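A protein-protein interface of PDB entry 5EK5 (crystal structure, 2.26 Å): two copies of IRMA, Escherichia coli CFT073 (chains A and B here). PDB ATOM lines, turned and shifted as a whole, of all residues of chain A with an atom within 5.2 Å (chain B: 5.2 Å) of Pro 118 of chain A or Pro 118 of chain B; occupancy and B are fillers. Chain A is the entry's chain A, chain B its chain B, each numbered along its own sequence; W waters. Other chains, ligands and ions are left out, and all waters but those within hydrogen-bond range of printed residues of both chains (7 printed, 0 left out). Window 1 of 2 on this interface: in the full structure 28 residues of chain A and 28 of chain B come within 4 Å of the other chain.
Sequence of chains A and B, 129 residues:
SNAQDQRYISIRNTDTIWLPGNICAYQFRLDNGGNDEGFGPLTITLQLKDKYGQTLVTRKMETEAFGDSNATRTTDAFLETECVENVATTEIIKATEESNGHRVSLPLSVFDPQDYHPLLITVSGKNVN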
ATOM      1  N   ASN A  13      23.508   2.230  -9.759  1.00  0.00           N
ATOM      2  CA  ASN A  13      22.518   3.189  -9.298  1.00  0.00           C
ATOM      3  C   ASN A  13      21.497   3.416 -10.404  1.00  0.00           C
ATOM      4  O   ASN A  13      21.867   3.741 -11.532  1.00  0.00           O
ATOM      5  CB  ASN A  13      23.195   4.498  -8.890  1.00  0.00           C
ATOM      6  CG  ASN A  13      22.210   5.620  -8.678  1.00  0.00           C
ATOM      7  OD1 ASN A  13      22.304   6.669  -9.309  1.00  0.00           O
ATOM      8  ND2 ASN A  13      21.244   5.399  -7.796  1.00  0.00           N
ATOM      9  N   ALA A  88      28.487  12.785  -6.530  1.00  0.00           N
ATOM     10  CA  ALA A  88      28.753  12.378  -7.902  1.00  0.00           C
ATOM     11  C   ALA A  88      28.991  10.880  -7.964  1.00  0.00           C
ATOM     12  O   ALA A  88      28.552  10.198  -8.886  1.00  0.00           O
ATOM     13  CB  ALA A  88      29.955  13.136  -8.461  1.00  0.00           C
ATOM     14  N   GLN A 114      29.132  -0.447 -11.133  1.00  0.00           N
ATOM     15  CA  GLN A 114      29.153   0.402 -12.319  1.00  0.00           C
ATOM     16  C   GLN A 114      30.095   1.579 -12.097  1.00  0.00           C
ATOM     17  O   GLN A 114      29.685   2.644 -11.623  1.00  0.00           O
ATOM     18  CB  GLN A 114      27.759   0.921 -12.677  1.00  0.00           C
ATOM     19  CG  GLN A 114      27.677   1.472 -14.104  1.00  0.00           C
ATOM     20  CD  GLN A 114      26.320   2.071 -14.444  1.00  0.00           C
ATOM     21  OE1 GLN A 114      25.545   2.430 -13.557  1.00  0.00           O
ATOM     22  NE2 GLN A 114      26.031   2.186 -15.735  1.00  0.00           N
ATOM     23  N   TYR A 116      31.467   3.556 -14.183  1.00  0.00           N
ATOM     24  CA  TYR A 116      31.463   4.217 -15.478  1.00  0.00           C
ATOM     25  C   TYR A 116      30.352   5.265 -15.534  1.00  0.00           C
ATOM     26  O   TYR A 116      29.247   5.031 -15.038  1.00  0.00           O
ATOM     27  CB  TYR A 116      31.289   3.157 -16.572  1.00  0.00           C
ATOM     28  CG  TYR A 116      30.862   3.659 -17.932  1.00  0.00           C
ATOM     29  CD1 TYR A 116      31.794   4.154 -18.835  1.00  0.00           C
ATOM     30  CD2 TYR A 116      29.531   3.599 -18.329  1.00  0.00           C
ATOM     31  CE1 TYR A 116      31.409   4.602 -20.084  1.00  0.00           C
ATOM     32  CE2 TYR A 116      29.138   4.037 -19.579  1.00  0.00           C
ATOM     33  CZ  TYR A 116      30.081   4.542 -20.451  1.00  0.00           C
ATOM     34  OH  TYR A 116      29.696   4.985 -21.692  1.00  0.00           O
ATOM     35  N   HIS A 117      30.658   6.426 -16.112  1.00  0.00           N
ATOM     36  CA  HIS A 117      29.661   7.470 -16.354  1.00  0.00           C
ATOM     37  C   HIS A 117      28.990   7.261 -17.705  1.00  0.00           C
ATOM     38  O   HIS A 117      29.619   7.451 -18.743  1.00  0.00           O
ATOM     39  CB  HIS A 117      30.294   8.863 -16.308  1.00  0.00           C
ATOM     40  CG  HIS A 117      30.708   9.304 -14.938  1.00  0.00           C
ATOM     41  ND1 HIS A 117      29.800   9.584 -13.943  1.00  0.00           N
ATOM     42  CD2 HIS A 117      31.933   9.532 -14.405  1.00  0.00           C
ATOM     43  CE1 HIS A 117      30.449   9.958 -12.845  1.00  0.00           C
ATOM     44  NE2 HIS A 117      31.743   9.931 -13.110  1.00  0.00           N
ATOM     45  N   PRO A 118      27.705   6.891 -17.702  1.00  0.00           N
ATOM     46  CA  PRO A 118      27.028   6.620 -18.974  1.00  0.00           C
ATOM     47  C   PRO A 118      26.490   7.859 -19.681  1.00  0.00           C
ATOM     48  O   PRO A 118      26.214   8.875 -19.037  1.00  0.00           O
ATOM     49  CB  PRO A 118      25.871   5.717 -18.553  1.00  0.00           C
ATOM     50  CG  PRO A 118      25.532   6.195 -17.188  1.00  0.00           C
ATOM     51  CD  PRO A 118      26.830   6.635 -16.546  1.00  0.00           C
ATOM     52  N   LEU A 119      26.339   7.759 -20.997  1.00  0.00           N
ATOM     53  CA  LEU A 119      25.602   8.759 -21.750  1.00  0.00           C
ATOM     54  C   LEU A 119      24.172   8.768 -21.249  1.00  0.00           C
ATOM     55  O   LEU A 119      23.598   7.715 -20.985  1.00  0.00           O
ATOM     56  CB  LEU A 119      25.623   8.470 -23.252  1.00  0.00           C
ATOM     57  CG  LEU A 119      26.948   8.459 -24.009  1.00  0.00           C
ATOM     58  CD1 LEU A 119      26.676   8.221 -25.483  1.00  0.00           C
ATOM     59  CD2 LEU A 119      27.700   9.764 -23.805  1.00  0.00           C
ATOM     60  N   LEU A 120      23.601   9.953 -21.114  1.00  0.00           N
ATOM     61  CA  LEU A 120      22.195  10.070 -20.787  1.00  0.00           C
ATOM     62  C   LEU A 120      21.376   9.858 -22.058  1.00  0.00           C
ATOM     63  O   LEU A 120      21.783  10.277 -23.144  1.00  0.00           O
ATOM     64  CB  LEU A 120      21.906  11.432 -20.160  1.00  0.00           C
ATOM     65  CG  LEU A 120      20.566  11.625 -19.455  1.00  0.00           C
ATOM     66  CD1 LEU A 120      20.757  12.452 -18.195  1.00  0.00           C
ATOM     67  CD2 LEU A 120      19.567  12.287 -20.384  1.00  0.00           C
ATOM     68  N   ASN B  13      23.167   3.216 -21.707  1.00  0.00           N
ATOM     69  CA  ASN B  13      24.538   3.159 -22.176  1.00  0.00           C
ATOM     70  C   ASN B  13      25.411   2.467 -21.137  1.00  0.00           C
ATOM     71  O   ASN B  13      25.433   2.863 -19.971  1.00  0.00           O
ATOM     72  CB  ASN B  13      25.054   4.566 -22.469  1.00  0.00           C
ATOM     73  CG  ASN B  13      26.545   4.603 -22.694  1.00  0.00           C
ATOM     74  OD1 ASN B  13      27.270   5.310 -21.993  1.00  0.00           O
ATOM     75  ND2 ASN B  13      27.014   3.851 -23.681  1.00  0.00           N
ATOM     76  N   ALA B  88      27.570  14.134 -24.409  1.00  0.00           N
ATOM     77  CA  ALA B  88      27.061  14.005 -23.046  1.00  0.00           C
ATOM     78  C   ALA B  88      25.737  13.243 -23.000  1.00  0.00           C
ATOM     79  O   ALA B  88      25.492  12.463 -22.078  1.00  0.00           O
ATOM     80  CB  ALA B  88      26.898  15.383 -22.410  1.00  0.00           C
ATOM     81  N   GLN B 114      17.477   5.539 -19.988  1.00  0.00           N
ATOM     82  CA  GLN B 114      18.145   6.071 -18.807  1.00  0.00           C
ATOM     83  C   GLN B 114      18.359   7.575 -18.954  1.00  0.00           C
ATOM     84  O   GLN B 114      19.412   8.008 -19.425  1.00  0.00           O
ATOM     85  CB  GLN B 114      19.479   5.357 -18.570  1.00  0.00           C
ATOM     86  CG  GLN B 114      20.018   5.570 -17.168  1.00  0.00           C
ATOM     87  CD  GLN B 114      21.347   4.891 -16.904  1.00  0.00           C
ATOM     88  OE1 GLN B 114      22.113   4.603 -17.822  1.00  0.00           O
ATOM     89  NE2 GLN B 114      21.612   4.605 -15.634  1.00  0.00           N
ATOM     90  N   TYR B 116      18.859   9.945 -16.730  1.00  0.00           N
ATOM     91  CA  TYR B 116      19.339  10.466 -15.460  1.00  0.00           C
ATOM     92  C   TYR B 116      20.817  10.152 -15.351  1.00  0.00           C
ATOM     93  O   TYR B 116      21.264   9.121 -15.848  1.00  0.00           O
ATOM     94  CB  TYR B 116      18.568   9.870 -14.280  1.00  0.00           C
ATOM     95  CG  TYR B 116      18.604   8.365 -14.257  1.00  0.00           C
ATOM     96  CD1 TYR B 116      19.656   7.684 -13.654  1.00  0.00           C
ATOM     97  CD2 TYR B 116      17.596   7.623 -14.856  1.00  0.00           C
ATOM     98  CE1 TYR B 116      19.700   6.312 -13.646  1.00  0.00           C
ATOM     99  CE2 TYR B 116      17.626   6.249 -14.847  1.00  0.00           C
ATOM    100  CZ  TYR B 116      18.684   5.600 -14.250  1.00  0.00           C
ATOM    101  OH  TYR B 116      18.712   4.223 -14.239  1.00  0.00           O
ATOM    102  N   HIS B 117      21.578  11.043 -14.731  1.00  0.00           N
ATOM    103  CA  HIS B 117      22.976  10.754 -14.453  1.00  0.00           C
ATOM    104  C   HIS B 117      23.054   9.944 -13.169  1.00  0.00           C
ATOM    105  O   HIS B 117      22.718  10.442 -12.091  1.00  0.00           O
ATOM    106  CB  HIS B 117      23.797  12.034 -14.320  1.00  0.00           C
ATOM    107  CG  HIS B 117      24.004  12.757 -15.621  1.00  0.00           C
ATOM    108  ND1 HIS B 117      24.768  12.248 -16.633  1.00  0.00           N
ATOM    109  CD2 HIS B 117      23.538  13.955 -16.047  1.00  0.00           C
ATOM    110  CE1 HIS B 117      24.773  13.101 -17.653  1.00  0.00           C
ATOM    111  NE2 HIS B 117      24.032  14.142 -17.315  1.00  0.00           N
ATOM    112  N   PRO B 118      23.467   8.675 -13.284  1.00  0.00           N
ATOM    113  CA  PRO B 118      23.537   7.817 -12.103  1.00  0.00           C
ATOM    114  C   PRO B 118      24.822   8.055 -11.332  1.00  0.00           C
ATOM    115  O   PRO B 118      25.805   8.529 -11.901  1.00  0.00           O
ATOM    116  CB  PRO B 118      23.511   6.412 -12.693  1.00  0.00           C
ATOM    117  CG  PRO B 118      24.202   6.567 -13.988  1.00  0.00           C
ATOM    118  CD  PRO B 118      23.859   7.952 -14.503  1.00  0.00           C
ATOM    119  N   LEU B 119      24.801   7.738 -10.044  1.00  0.00           N
ATOM    120  CA  LEU B 119      26.015   7.731  -9.252  1.00  0.00           C
ATOM    121  C   LEU B 119      26.986   6.702  -9.801  1.00  0.00           C
ATOM    122  O   LEU B 119      26.596   5.589 -10.151  1.00  0.00           O
ATOM    123  CB  LEU B 119      25.699   7.429  -7.787  1.00  0.00           C
ATOM    124  CG  LEU B 119      24.788   8.430  -7.075  1.00  0.00           C
ATOM    125  CD1 LEU B 119      24.619   8.047  -5.615  1.00  0.00           C
ATOM    126  CD2 LEU B 119      25.340   9.842  -7.208  1.00  0.00           C
ATOM    127  N   LEU B 120      28.255   7.072  -9.874  1.00  0.00           N
ATOM    128  CA  LEU B 120      29.277   6.107 -10.221  1.00  0.00           C
ATOM    129  C   LEU B 120      29.586   5.314  -8.958  1.00  0.00           C
ATOM    130  O   LEU B 120      29.600   5.867  -7.858  1.00  0.00           O
ATOM    131  CB  LEU B 120      30.522   6.800 -10.777  1.00  0.00           C
ATOM    132  CG  LEU B 120      31.549   5.898 -11.461  1.00  0.00           C
ATOM    133  CD1 LEU B 120      32.112   6.574 -12.698  1.00  0.00           C
ATOM    134  CD2 LEU B 120      32.666   5.560 -10.491  1.00  0.00           C
HETATM  135  O   HOH W   1      23.704   2.747 -17.450  1.00  0.00           O
HETATM  136  O   HOH W   2      22.344   5.360 -20.231  1.00  0.00           O
HETATM  137  O   HOH W   3      25.556   3.335 -11.168  1.00  0.00           O
HETATM  138  O   HOH W   4      22.902   2.712 -14.008  1.00  0.00           O
HETATM  139  O   HOH W   5      27.033   9.260 -14.234  1.00  0.00           O
HETATM  140  O   HOH W   6      26.125  10.105 -16.707  1.00  0.00           O
HETATM  141  O   HOH W   7      27.736  10.902 -11.263  1.00  0.00           O
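Water W1 lies within hydrogen-bond range of OE1 of Gln 114 of chain B (2.5 Å), NE2 of Gln 114 of chain A (2.9 Å) and O of Asn 13 of chain B (3.1 Å).
Water W2 lies within hydrogen-bond range of the side-chain amide oxygen (OE1) of Gln 114 of chain B (2.5 Å), the backbone NH (N) of Asn 13 of chain B (2.7 Å) and the backbone carbonyl oxygen (O) of Leu 119 of chain A (2.8 Å).
Water W6 lies within hydrogen-bond range of a ring nitrogen (ND1) of His 117 of chain B (2.5 Å) and the backbone carbonyl oxygen (O) of Pro 118 of chain A (2.6 Å).
Water W3 lies within hydrogen-bond range of the side-chain amide oxygen (OE1) of Gln 114 of chain A (2.6 Å), the backbone carbonyl oxygen (O) of Leu 119 of chain B (2.7 Å) and the backbone NH (N) of Asn 13 of chain A (2.7 Å).
Water W7 bridges the backbone carbonyl oxygen of Ala 88 of chain A and the backbone carbonyl oxygen of Pro 118 of chain B.
Water W5 bridges the backbone carbonyl oxygen (O) of Pro 118 of chain B (2.7 Å) and a ring nitrogen (ND1) of His 117 of chain A (2.8 Å).
Among the printed residues, pairs that only touch across the chains: Asn 13 of chain A with Tyr 116 of chain B (3.97 Å), Asn 13 of chain A with Pro 118 of chain B (3.3 Å), Ala 88 of chain A with Leu 119 of chain B (3.6 Å), Gln 114 of chain A with Leu 120 of chain B (3.8 Å), Tyr 116 of chain A with Leu 120 of chain B (3.4 Å), His 117 of chain A with Leu 120 of chain B (3.4 Å), Pro 118 of chain A with Asn 13 of chain B (3.2 Å), Pro 118 of chain A with Gln 114 of chain B (3.8 Å), Pro 118 of chain A with Pro 118 of chain B (3.5 Å), Leu 119 of chain A with Ala 88 of chain B (3.7 Å), Leu 120 of chain A with Gln 114 of chain B (3.7 Å), Leu 120 of chain A with Tyr 116 of chain B (3.5 Å) and Leu 120 of chain A with His 117 of chain B (3.8 Å).
Asn 13 of chain A touches Leu 119 of chain B, and with the chains exchanged Leu 119 of chain A touches Asn 13 of chain B.
Tyr 116 of chain A touches Leu 120 of chain B, and with the chains exchanged Leu 120 of chain A touches Tyr 116 of chain B.
His 117 of chain A touches Leu 120 of chain B, and with the chains exchanged Leu 120 of chain A touches His 117 of chain B.
Pro 118 of chain A touches Gln 114 of chain B, but with the chains exchanged Gln 114 of chain A does not touch Pro 118 of chain B (4.4 Å).
The side-chain amide oxygen (OD1) of Asn 13 of chain A lies within hydrogen-bond range of the backbone NH (N) of Leu 119 of chain B (2.8 Å).
The backbone carbonyl oxygen (O) of Ala 88 of chain A lies within hydrogen-bond range of the backbone NH (N) of Leu 120 of chain B (3.3 Å).
The side-chain amide oxygen (OD1) of Asn 13 of chain B sits at hydrogen-bond distance from the side-chain hydroxyl (OH) of Tyr 116 of chain A (2.5 Å).
The side-chain amide oxygen (OD1) of Asn 13 of chain B lies within hydrogen-bond range of the backbone NH (N) of Leu 119 of chain A (2.8 Å).
The backbone NH of Leu 120 of chain A lies within hydrogen-bond range of the backbone carbonyl oxygen of Ala 88 of chain B.
Of the 8 printed residues of chain B, 8 touch a printed residue of chain A.
Printed residues of chain B that touch a printed residue of chain A: Asn 13, Ala 88, Gln 114, Tyr 116, His 117, Pro 118, Leu 119 and Leu 120.
Hydrophobic or aromatic side chains of chain B within 4 Å of the printed part of chain A: Tyr 116, His 117, Pro 118, Leu 119 and Leu 120.
Hydrophobic or aromatic side chains of chain A that line the printed part of chain B: Tyr 116, His 117, Pro 118, Leu 119 and Leu 120.
Along chain A the printed residues that touch a printed residue of chain B span positions 13 to 120.
Among the printed residues, no Asp or Glu carboxylate lies within 4 Å of a Lys or Arg side-chain nitrogen of the other chain.
Printed residues of chain B within 4 Å of Asn 13 of chain A: Tyr 116 (3.97 Å), Pro 118 (3.3 Å) and Leu 119 (2.8 Å).
Of the printed residues of chain B, Tyr 116 of chain A touches Asn 13 and Leu 120.
Of the printed residues of chain B, His 117 of chain A touches Leu 120.
Of chain B, only Asn 13, Gln 114 and Pro 118 come within 4 Å of Pro 118 of chain A.
Of the printed residues of chain A, Gln 114 of chain B touches Pro 118 and Leu 120.
Of the printed residues of chain A, His 117 of chain B touches Leu 120.
Of the printed residues of chain A, Pro 118 of chain B touches Asn 13 (3.3 Å) and Pro 118 (3.5 Å).
The nearest residue of chain A that does not touch Pro 118 of chain B is Gln 114 of chain A (4.4 Å).
OH of Tyr 116 of chain B lies within hydrogen-bond range of NE2 of Gln 114 of chain B, 3.2 Å away.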
